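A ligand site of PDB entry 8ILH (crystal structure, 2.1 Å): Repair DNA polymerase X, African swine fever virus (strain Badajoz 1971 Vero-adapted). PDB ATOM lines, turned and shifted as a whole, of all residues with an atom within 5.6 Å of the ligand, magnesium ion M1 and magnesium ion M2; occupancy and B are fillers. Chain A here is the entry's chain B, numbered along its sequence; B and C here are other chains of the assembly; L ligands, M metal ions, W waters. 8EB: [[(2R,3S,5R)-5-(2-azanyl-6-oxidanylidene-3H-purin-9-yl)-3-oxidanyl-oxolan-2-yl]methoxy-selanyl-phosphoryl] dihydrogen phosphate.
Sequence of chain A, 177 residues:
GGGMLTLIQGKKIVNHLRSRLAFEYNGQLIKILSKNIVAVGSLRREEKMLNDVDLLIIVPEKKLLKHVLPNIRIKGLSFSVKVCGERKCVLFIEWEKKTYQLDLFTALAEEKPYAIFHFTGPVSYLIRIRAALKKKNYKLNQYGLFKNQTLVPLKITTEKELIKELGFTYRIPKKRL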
ATOM      1  N   GLY A  41      -4.078  12.992  -7.269  1.00  0.00           N
ATOM      2  CA  GLY A  41      -3.608  11.665  -7.653  1.00  0.00           C
ATOM      3  C   GLY A  41      -4.178  10.526  -6.816  1.00  0.00           C
ATOM      4  O   GLY A  41      -5.238  10.671  -6.192  1.00  0.00           O
ATOM      5  N   SER A  42      -3.472   9.401  -6.806  1.00  0.00           N
ATOM      6  CA  SER A  42      -3.948   8.185  -6.113  1.00  0.00           C
ATOM      7  C   SER A  42      -4.099   8.385  -4.595  1.00  0.00           C
ATOM      8  O   SER A  42      -4.946   7.733  -3.976  1.00  0.00           O
ATOM      9  CB  SER A  42      -3.066   6.971  -6.433  1.00  0.00           C
ATOM     10  OG  SER A  42      -1.723   7.155  -6.022  1.00  0.00           O
ATOM     11  N   LEU A  43      -3.296   9.288  -4.029  1.00  0.00           N
ATOM     12  CA  LEU A  43      -3.405   9.647  -2.615  1.00  0.00           C
ATOM     13  C   LEU A  43      -4.784  10.216  -2.289  1.00  0.00           C
ATOM     14  O   LEU A  43      -5.391   9.819  -1.307  1.00  0.00           O
ATOM     15  CB  LEU A  43      -2.329  10.659  -2.237  1.00  0.00           C
ATOM     16  CG  LEU A  43      -2.083  10.870  -0.703  1.00  0.00           C
ATOM     17  CD1 LEU A  43      -0.664  11.296  -0.346  1.00  0.00           C
ATOM     18  CD2 LEU A  43      -3.023  11.918  -0.135  1.00  0.00           C
ATOM     19  N   ARG A  45      -7.441   9.692  -4.079  1.00  0.00           N
ATOM     20  CA  ARG A  45      -8.327   8.557  -4.322  1.00  0.00           C
ATOM     21  C   ARG A  45      -8.248   7.463  -3.229  1.00  0.00           C
ATOM     22  O   ARG A  45      -8.997   6.492  -3.296  1.00  0.00           O
ATOM     23  CB  ARG A  45      -8.057   7.959  -5.711  1.00  0.00           C
ATOM     24  CG  ARG A  45      -8.371   8.918  -6.862  1.00  0.00           C
ATOM     25  CD  ARG A  45      -8.517   8.191  -8.187  1.00  0.00           C
ATOM     26  NE  ARG A  45      -7.457   7.197  -8.438  1.00  0.00           N
ATOM     27  CZ  ARG A  45      -6.254   7.454  -8.958  1.00  0.00           C
ATOM     28  NH1 ARG A  45      -5.877   8.689  -9.303  1.00  0.00           N
ATOM     29  NH2 ARG A  45      -5.391   6.444  -9.121  1.00  0.00           N
ATOM     30  N   ASN A  51       2.430   4.827  -5.967  1.00  0.00           N
ATOM     31  CA  ASN A  51       3.684   4.922  -6.718  1.00  0.00           C
ATOM     32  C   ASN A  51       4.431   6.214  -6.446  1.00  0.00           C
ATOM     33  O   ASN A  51       5.637   6.284  -6.656  1.00  0.00           O
ATOM     34  CB  ASN A  51       3.482   4.682  -8.205  1.00  0.00           C
ATOM     35  CG  ASN A  51       3.400   3.230  -8.520  1.00  0.00           C
ATOM     36  OD1 ASN A  51       4.386   2.501  -8.370  1.00  0.00           O
ATOM     37  ND2 ASN A  51       2.231   2.777  -8.928  1.00  0.00           N
ATOM     38  N   ASP A  52       3.705   7.240  -5.994  1.00  0.00           N
ATOM     39  CA  ASP A  52       4.276   8.550  -5.688  1.00  0.00           C
ATOM     40  C   ASP A  52       3.263   9.410  -4.923  1.00  0.00           C
ATOM     41  O   ASP A  52       2.145   8.979  -4.670  1.00  0.00           O
ATOM     42  CB  ASP A  52       4.686   9.240  -6.986  1.00  0.00           C
ATOM     43  CG  ASP A  52       3.590   9.169  -8.018  1.00  0.00           C
ATOM     44  OD1 ASP A  52       2.509   9.737  -7.769  1.00  0.00           O
ATOM     45  OD2 ASP A  52       3.811   8.490  -9.055  1.00  0.00           O
ATOM     46  N   VAL A  53       3.689  10.621  -4.563  1.00  0.00           N
ATOM     47  CA  VAL A  53       2.816  11.620  -3.962  1.00  0.00           C
ATOM     48  C   VAL A  53       2.602  12.761  -4.965  1.00  0.00           C
ATOM     49  O   VAL A  53       3.572  13.296  -5.498  1.00  0.00           O
ATOM     50  CB  VAL A  53       3.428  12.160  -2.651  1.00  0.00           C
ATOM     51  CG1 VAL A  53       2.546  13.234  -2.031  1.00  0.00           C
ATOM     52  CG2 VAL A  53       3.645  11.041  -1.658  1.00  0.00           C
ATOM     53  N   ASP A  54       1.344  13.125  -5.182  1.00  0.00           N
ATOM     54  CA  ASP A  54       0.979  14.203  -6.115  1.00  0.00           C
ATOM     55  C   ASP A  54       0.386  15.377  -5.359  1.00  0.00           C
ATOM     56  O   ASP A  54      -0.579  15.219  -4.624  1.00  0.00           O
ATOM     57  CB  ASP A  54      -0.053  13.705  -7.117  1.00  0.00           C
ATOM     58  CG  ASP A  54       0.426  12.524  -7.892  1.00  0.00           C
ATOM     59  OD1 ASP A  54       1.454  12.641  -8.589  1.00  0.00           O
ATOM     60  OD2 ASP A  54      -0.201  11.453  -7.825  1.00  0.00           O
ATOM     61  N   GLN A 101       9.137   9.451  -4.972  1.00  0.00           N
ATOM     62  CA  GLN A 101       8.832  10.413  -6.015  1.00  0.00           C
ATOM     63  C   GLN A 101       7.720  11.343  -5.547  1.00  0.00           C
ATOM     64  O   GLN A 101       6.669  10.887  -5.096  1.00  0.00           O
ATOM     65  CB  GLN A 101       8.414   9.699  -7.299  1.00  0.00           C
ATOM     66  CG  GLN A 101       8.164  10.671  -8.450  1.00  0.00           C
ATOM     67  CD  GLN A 101       8.077   9.990  -9.804  1.00  0.00           C
ATOM     68  OE1 GLN A 101       8.910   9.139 -10.131  1.00  0.00           O
ATOM     69  NE2 GLN A 101       7.090  10.385 -10.606  1.00  0.00           N
ATOM     70  N   ASP A 103       5.483  14.457  -7.080  1.00  0.00           N
ATOM     71  CA  ASP A 103       5.081  15.178  -8.279  1.00  0.00           C
ATOM     72  C   ASP A 103       4.337  16.457  -7.915  1.00  0.00           C
ATOM     73  O   ASP A 103       3.321  16.425  -7.219  1.00  0.00           O
ATOM     74  CB  ASP A 103       4.204  14.297  -9.168  1.00  0.00           C
ATOM     75  CG  ASP A 103       4.982  13.172  -9.831  1.00  0.00           C
ATOM     76  OD1 ASP A 103       6.237  13.209  -9.769  1.00  0.00           O
ATOM     77  OD2 ASP A 103       4.353  12.262 -10.397  1.00  0.00           O
ATOM     78  N   PHE A 105       2.470  20.000  -9.286  1.00  0.00           N
ATOM     79  CA  PHE A 105       1.793  20.665 -10.405  1.00  0.00           C
ATOM     80  C   PHE A 105       1.274  22.030  -9.975  1.00  0.00           C
ATOM     81  O   PHE A 105       1.003  22.234  -8.783  1.00  0.00           O
ATOM     82  CB  PHE A 105       0.632  19.806 -10.880  1.00  0.00           C
ATOM     83  CG  PHE A 105       1.005  18.385 -11.155  1.00  0.00           C
ATOM     84  CD1 PHE A 105       1.636  18.040 -12.343  1.00  0.00           C
ATOM     85  CD2 PHE A 105       0.737  17.383 -10.225  1.00  0.00           C
ATOM     86  CE1 PHE A 105       1.986  16.719 -12.607  1.00  0.00           C
ATOM     87  CE2 PHE A 105       1.077  16.063 -10.479  1.00  0.00           C
ATOM     88  CZ  PHE A 105       1.712  15.732 -11.665  1.00  0.00           C
ATOM     89  N   HIS A 118      -8.840  17.057 -13.089  1.00  0.00           N
ATOM     90  CA  HIS A 118      -7.825  16.405 -13.905  1.00  0.00           C
ATOM     91  C   HIS A 118      -6.817  15.600 -13.067  1.00  0.00           C
ATOM     92  O   HIS A 118      -6.630  14.411 -13.302  1.00  0.00           O
ATOM     93  CB  HIS A 118      -7.096  17.436 -14.789  1.00  0.00           C
ATOM     94  CG  HIS A 118      -5.857  16.908 -15.467  1.00  0.00           C
ATOM     95  ND1 HIS A 118      -5.852  16.440 -16.756  1.00  0.00           N
ATOM     96  CD2 HIS A 118      -4.578  16.828 -15.036  1.00  0.00           C
ATOM     97  CE1 HIS A 118      -4.629  16.056 -17.085  1.00  0.00           C
ATOM     98  NE2 HIS A 118      -3.833  16.288 -16.052  1.00  0.00           N
ATOM     99  N   PHE A 119      -6.159  16.259 -12.107  1.00  0.00           N
ATOM    100  CA  PHE A 119      -5.093  15.606 -11.336  1.00  0.00           C
ATOM    101  C   PHE A 119      -5.579  14.556 -10.322  1.00  0.00           C
ATOM    102  O   PHE A 119      -4.779  13.765  -9.837  1.00  0.00           O
ATOM    103  CB  PHE A 119      -4.187  16.629 -10.659  1.00  0.00           C
ATOM    104  CG  PHE A 119      -3.327  17.378 -11.619  1.00  0.00           C
ATOM    105  CD1 PHE A 119      -2.284  16.727 -12.259  1.00  0.00           C
ATOM    106  CD2 PHE A 119      -3.586  18.709 -11.943  1.00  0.00           C
ATOM    107  CE1 PHE A 119      -1.500  17.404 -13.182  1.00  0.00           C
ATOM    108  CE2 PHE A 119      -2.798  19.392 -12.853  1.00  0.00           C
ATOM    109  CZ  PHE A 119      -1.748  18.731 -13.475  1.00  0.00           C
ATOM    110  N   THR A 120      -6.873  14.530 -10.027  1.00  0.00           N
ATOM    111  CA  THR A 120      -7.444  13.445  -9.228  1.00  0.00           C
ATOM    112  C   THR A 120      -7.518  12.129  -9.994  1.00  0.00           C
ATOM    113  O   THR A 120      -7.307  11.059  -9.411  1.00  0.00           O
ATOM    114  CB  THR A 120      -8.826  13.837  -8.698  1.00  0.00           C
ATOM    115  OG1 THR A 120      -8.663  14.962  -7.836  1.00  0.00           O
ATOM    116  CG2 THR A 120      -9.470  12.698  -7.903  1.00  0.00           C
ATOM    117  N   GLY A 121      -7.813  12.196 -11.292  1.00  0.00           N
ATOM    118  CA  GLY A 121      -7.965  10.990 -12.091  1.00  0.00           C
ATOM    119  C   GLY A 121      -9.094  10.114 -11.540  1.00  0.00           C
ATOM    120  O   GLY A 121     -10.065  10.639 -11.010  1.00  0.00           O
ATOM    121  N   PRO A 122      -8.998   8.786 -11.673  1.00  0.00           N
ATOM    122  CA  PRO A 122      -7.931   8.086 -12.411  1.00  0.00           C
ATOM    123  C   PRO A 122      -7.990   8.323 -13.913  1.00  0.00           C
ATOM    124  O   PRO A 122      -8.990   8.845 -14.432  1.00  0.00           O
ATOM    125  CB  PRO A 122      -8.229   6.623 -12.101  1.00  0.00           C
ATOM    126  CG  PRO A 122      -9.707   6.576 -11.991  1.00  0.00           C
ATOM    127  CD  PRO A 122     -10.119   7.884 -11.368  1.00  0.00           C
ATOM    128  N   VAL A 123      -6.945   7.881 -14.604  1.00  0.00           N
ATOM    129  CA  VAL A 123      -6.795   8.135 -16.046  1.00  0.00           C
ATOM    130  C   VAL A 123      -7.986   7.565 -16.844  1.00  0.00           C
ATOM    131  O   VAL A 123      -8.570   8.264 -17.670  1.00  0.00           O
ATOM    132  CB  VAL A 123      -5.440   7.603 -16.581  1.00  0.00           C
ATOM    133  CG1 VAL A 123      -5.322   7.797 -18.084  1.00  0.00           C
ATOM    134  CG2 VAL A 123      -4.291   8.317 -15.897  1.00  0.00           C
ATOM    135  N   LEU A 126     -11.024   9.815 -16.638  1.00  0.00           N
ATOM    136  CA  LEU A 126     -10.850  11.034 -17.435  1.00  0.00           C
ATOM    137  C   LEU A 126     -11.065  10.761 -18.920  1.00  0.00           C
ATOM    138  O   LEU A 126     -11.736  11.536 -19.594  1.00  0.00           O
ATOM    139  CB  LEU A 126      -9.468  11.635 -17.231  1.00  0.00           C
ATOM    140  CG  LEU A 126      -9.110  12.113 -15.820  1.00  0.00           C
ATOM    141  CD1 LEU A 126      -7.707  12.690 -15.859  1.00  0.00           C
ATOM    142  CD2 LEU A 126     -10.095  13.131 -15.290  1.00  0.00           C
ATOM    143  N   ARG A 130     -13.889  12.596 -21.008  1.00  0.00           N
ATOM    144  CA  ARG A 130     -13.428  13.438 -22.093  1.00  0.00           C
ATOM    145  C   ARG A 130     -13.961  12.971 -23.458  1.00  0.00           C
ATOM    146  O   ARG A 130     -14.322  13.792 -24.306  1.00  0.00           O
ATOM    147  CB  ARG A 130     -11.900  13.543 -22.075  1.00  0.00           C
ATOM    148  CG  ARG A 130     -11.421  14.383 -20.911  1.00  0.00           C
ATOM    149  CD  ARG A 130      -9.926  14.324 -20.670  1.00  0.00           C
ATOM    150  NE  ARG A 130      -9.628  15.252 -19.587  1.00  0.00           N
ATOM    151  CZ  ARG A 130      -8.472  15.878 -19.368  1.00  0.00           C
ATOM    152  NH1 ARG A 130      -7.396  15.689 -20.137  1.00  0.00           N
ATOM    153  NH2 ARG A 130      -8.406  16.715 -18.346  1.00  0.00           N
ATOM    154  P    DC B   7       6.243   9.974 -14.804  1.00  0.00           P
ATOM    155  OP1  DC B   7       7.202  10.291 -13.775  1.00  0.00           O
ATOM    156  OP2  DC B   7       5.732   8.620 -14.926  1.00  0.00           O
ATOM    157  O5'  DC B   7       4.890  10.810 -14.791  1.00  0.00           O
ATOM    158  C5'  DC B   7       4.879  12.145 -14.280  1.00  0.00           C
ATOM    159  C4'  DC B   7       3.554  12.820 -14.532  1.00  0.00           C
ATOM    160  O4'  DC B   7       3.338  13.023 -15.935  1.00  0.00           O
ATOM    161  C3'  DC B   7       2.323  12.058 -14.089  1.00  0.00           C
ATOM    162  O3'  DC B   7       2.106  12.094 -12.689  1.00  0.00           O
ATOM    163  C2'  DC B   7       1.247  12.828 -14.828  1.00  0.00           C
ATOM    164  C1'  DC B   7       1.940  13.186 -16.137  1.00  0.00           C
ATOM    165  N1   DC B   7       1.538  12.330 -17.253  1.00  0.00           N
ATOM    166  C2   DC B   7       0.485  12.770 -18.048  1.00  0.00           C
ATOM    167  O2   DC B   7      -0.055  13.838 -17.779  1.00  0.00           O
ATOM    168  N3   DC B   7       0.065  11.999 -19.076  1.00  0.00           N
ATOM    169  C4   DC B   7       0.659  10.828 -19.316  1.00  0.00           C
ATOM    170  N4   DC B   7       0.216  10.105 -20.335  1.00  0.00           N
ATOM    171  C5   DC B   7       1.736  10.352 -18.513  1.00  0.00           C
ATOM    172  C6   DC B   7       2.129  11.123 -17.500  1.00  0.00           C
ATOM    173  O5'  DC C   1      -9.751   9.887 -26.342  1.00  0.00           O
ATOM    174  C5'  DC C   1     -10.655  10.251 -25.283  1.00  0.00           C
ATOM    175  C4'  DC C   1     -10.219  11.536 -24.608  1.00  0.00           C
ATOM    176  O4'  DC C   1      -9.332  11.256 -23.485  1.00  0.00           O
ATOM    177  C3'  DC C   1      -9.517  12.572 -25.479  1.00  0.00           C
ATOM    178  O3'  DC C   1     -10.161  13.831 -25.263  1.00  0.00           O
ATOM    179  C2'  DC C   1      -8.067  12.507 -25.024  1.00  0.00           C
ATOM    180  C1'  DC C   1      -8.170  12.058 -23.575  1.00  0.00           C
ATOM    181  N1   DC C   1      -7.020  11.247 -23.094  1.00  0.00           N
ATOM    182  C2   DC C   1      -6.331  11.642 -21.933  1.00  0.00           C
ATOM    183  O2   DC C   1      -6.697  12.669 -21.331  1.00  0.00           O
ATOM    184  N3   DC C   1      -5.296  10.891 -21.494  1.00  0.00           N
ATOM    185  C4   DC C   1      -4.934   9.797 -22.170  1.00  0.00           C
ATOM    186  N4   DC C   1      -3.901   9.089 -21.700  1.00  0.00           N
ATOM    187  C5   DC C   1      -5.620   9.374 -23.343  1.00  0.00           C
ATOM    188  C6   DC C   1      -6.649  10.114 -23.764  1.00  0.00           C
ATOM    189  P    DG C   2      -9.890  15.118 -26.205  1.00  0.00           P
ATOM    190  OP1  DG C   2     -11.046  16.024 -26.032  1.00  0.00           O
ATOM    191  OP2  DG C   2      -9.486  14.652 -27.554  1.00  0.00           O
ATOM    192  O5'  DG C   2      -8.608  15.785 -25.523  1.00  0.00           O
ATOM    193  C5'  DG C   2      -8.733  16.376 -24.221  1.00  0.00           C
ATOM    194  C4'  DG C   2      -7.380  16.759 -23.684  1.00  0.00           C
ATOM    195  O4'  DG C   2      -6.659  15.576 -23.262  1.00  0.00           O
ATOM    196  C3'  DG C   2      -6.447  17.499 -24.661  1.00  0.00           C
ATOM    197  O3'  DG C   2      -6.238  18.807 -24.129  1.00  0.00           O
ATOM    198  C2'  DG C   2      -5.209  16.630 -24.730  1.00  0.00           C
ATOM    199  C1'  DG C   2      -5.289  15.859 -23.435  1.00  0.00           C
ATOM    200  N9   DG C   2      -4.549  14.600 -23.401  1.00  0.00           N
ATOM    201  C8   DG C   2      -4.547  13.593 -24.329  1.00  0.00           C
ATOM    202  N7   DG C   2      -3.741  12.611 -24.026  1.00  0.00           N
ATOM    203  C5   DG C   2      -3.185  12.990 -22.813  1.00  0.00           C
ATOM    204  C6   DG C   2      -2.244  12.327 -21.993  1.00  0.00           C
ATOM    205  O6   DG C   2      -1.692  11.234 -22.167  1.00  0.00           O
ATOM    206  N1   DG C   2      -1.949  13.069 -20.853  1.00  0.00           N
ATOM    207  C2   DG C   2      -2.481  14.292 -20.542  1.00  0.00           C
ATOM    208  N2   DG C   2      -2.069  14.859 -19.399  1.00  0.00           N
ATOM    209  N3   DG C   2      -3.370  14.923 -21.307  1.00  0.00           N
ATOM    210  C4   DG C   2      -3.668  14.224 -22.417  1.00  0.00           C
HETATM  211  O3B 8EB L   1      -1.417   6.779 -10.375  1.00  0.00           O
HETATM  212  PB  8EB L   1      -1.946   8.294 -10.247  1.00  0.00           P
HETATM  213  O1B 8EB L   1      -3.459   8.206 -10.331  1.00  0.00           O
HETATM  214  O2B 8EB L   1      -1.348   8.863  -8.983  1.00  0.00           O
HETATM  215  O3A 8EB L   1      -1.354   9.009 -11.600  1.00  0.00           O
HETATM  216  PA  8EB L   1       0.056   9.777 -11.930  1.00  0.00           P
HETATM  217  O1A 8EB L   1       0.767   9.119 -13.109  1.00  0.00           O
HETATM  218  O5' 8EB L   1      -0.411  11.274 -12.313  1.00  0.00           O
HETATM  219  C5' 8EB L   1      -1.130  12.078 -11.394  1.00  0.00           C
HETATM  220  C4' 8EB L   1      -2.476  12.507 -11.964  1.00  0.00           C
HETATM  221  O4' 8EB L   1      -2.312  13.166 -13.218  1.00  0.00           O
HETATM  222  C3' 8EB L   1      -3.449  11.380 -12.234  1.00  0.00           C
HETATM  223  O3' 8EB L   1      -4.155  10.927 -11.072  1.00  0.00           O
HETATM  224  C2' 8EB L   1      -4.377  12.019 -13.246  1.00  0.00           C
HETATM  225  C1' 8EB L   1      -3.407  12.847 -14.072  1.00  0.00           C
HETATM  226  N9  8EB L   1      -2.943  12.044 -15.229  1.00  0.00           N
HETATM  227  C8  8EB L   1      -1.940  11.147 -15.235  1.00  0.00           C
HETATM  228  N7  8EB L   1      -1.770  10.575 -16.446  1.00  0.00           N
HETATM  229  C5  8EB L   1      -2.710  11.110 -17.235  1.00  0.00           C
HETATM  230  C6  8EB L   1      -3.114  10.942 -18.631  1.00  0.00           C
HETATM  231  N1  8EB L   1      -4.140  11.670 -19.088  1.00  0.00           N
HETATM  232  C2  8EB L   1      -4.816  12.548 -18.316  1.00  0.00           C
HETATM  233  N2  8EB L   1      -5.850  13.269 -18.839  1.00  0.00           N
HETATM  234  N3  8EB L   1      -4.494  12.744 -17.004  1.00  0.00           N
HETATM  235  C4  8EB L   1      -3.482  12.069 -16.431  1.00  0.00           C
HETATM  236  O6  8EB L   1      -2.483  10.144 -19.361  1.00  0.00           O
HETATM  237 SEA  8EB L   1       1.126  10.028 -10.427  1.00  0.00          SE
HETATM  238 MG    MG M   1       0.440   9.455  -8.462  1.00  0.00          MG
HETATM  239 MG    MG M   2       2.528  11.487  -9.794  1.00  0.00          MG
HETATM  240  O   HOH W   1      -1.248  15.317 -15.621  1.00  0.00           O
HETATM  241  O   HOH W   2       2.962   8.355 -15.688  1.00  0.00           O
HETATM  242  O   HOH W   3      -0.154   8.999  -6.606  1.00  0.00           O
HETATM  243  O   HOH W   4       0.146   8.263 -16.551  1.00  0.00           O
HETATM  244  O   HOH W   5      -4.107   7.092 -12.667  1.00  0.00           O
HETATM  245  O   HOH W   6       1.241   7.083  -8.945  1.00  0.00           O
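Magnesium ion M1 is bound by O2B of the ligand, water W3, SEA of the ligand, OD2 of Asp 54, OD1 of Asp 52 and water W6.
Water W6 lies within hydrogen-bond range of the side-chain carboxylate of Asp 52 (2.9 Å) and an oxygen (O3B) of the ligand (3.0 Å).
Water W3 lies within hydrogen-bond range of OG of Ser 42 (2.5 Å) and O of Asp 52 (3.0 Å).
Water W1 lies within hydrogen-bond range of a ring nitrogen (NE2) of His 118, O2 of DC 7 of chain B and an oxygen (O4') of the ligand.
Water W2 lies within hydrogen-bond range of OP2 of DC 7 of chain B (2.9 Å) and an oxygen (O1A) of the ligand (3.5 Å).
Merely in contact with magnesium ion M1: Ser 42 (3.99 Å).
Three residues have an atom within 4 Å of magnesium ion M1: Ser 42, Asp 52 and Asp 54.
O2 of DC 1 of chain C is in hydrogen-bond range of the guanidinium group (NH1) of Arg 130 (3.3 Å).
O of Phe 119 lies within hydrogen-bond range of N of Gly 41.
The side-chain carboxylate of Asp 103 is in hydrogen-bond range of the side-chain amide nitrogen of Gln 101, 3.1 Å away.
The backbone NH (N) of Asp 103 sits at hydrogen-bond distance from the backbone carbonyl oxygen (O) of Val 53 (2.7 Å).
The guanidinium group (NH1) of Arg 130 sits at hydrogen-bond distance from O4' of DG 2 of chain C (3.2 Å).
NE2 of Gln 101 sits at hydrogen-bond distance from OP1 of DC 7 of chain B.
ND1 of His 118 is in hydrogen-bond range of NH2 of Arg 130 (3.0 Å).
O of Thr 120 is in hydrogen-bond range of NH1 of Arg 45, at 2.8 Å.
Magnesium ion M2 is bound by OD1 of Asp 54 (2.0 Å), OD2 of Asp 103 (2.1 Å) and SEA of the ligand (2.1 Å).
Magnesium ion M2 has three donor atoms within binding distance.
Slightly farther from magnesium ion M2 lies OD1 of Asp 52 (2.7 Å).
N2 of the ligand lies close to NH1 of Arg 130.
O6 of DG 2 of chain C sits close to an oxygen (O6) of the ligand (3.1 Å).
Residues that only touch the ligand: Gly 41 (3.5 Å), His 118 (3.3 Å), Thr 120 (3.6 Å), Gly 121 (3.9 Å), Val 123 (3.4 Å) and Leu 126 (3.4 Å).
16 residues have an atom within 4 Å of the ligand: Gly 41, Ser 42, Arg 45, Asp 52, Asp 54, Asp 103, His 118, Phe 119, Thr 120, Gly 121, Val 123, Leu 126, Arg 130, DC 7 of chain B, DC 1 of chain C and DG 2 of chain C.
O3' of DC 7 of chain B lies close to O5' of the ligand (2.7 Å).
O2 of DC 1 of chain C lies within hydrogen-bond range of a nitrogen (N2) of the ligand (2.7 Å).
O2B of the ligand lies close to N of Ser 42, at 3.1 Å.
NH1 of Arg 45 is in salt-bridge range of O1B of the ligand (2.7 Å).
O of Phe 119 lies within hydrogen-bond range of O3' of the ligand (3.2 Å).
The side-chain hydroxyl (OG) of Ser 42 lies close to an oxygen (O2B) of the ligand (3.4 Å).
Merely in contact with magnesium ion M2: DC 7 of chain B (3.0 Å).
Within 4 Å of magnesium ion M2: Asp 52, Asp 54, Asp 103 and DC 7 of chain B.
The nearest printed residue that does not touch magnesium ion M2 is Phe 105 (4.7 Å).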
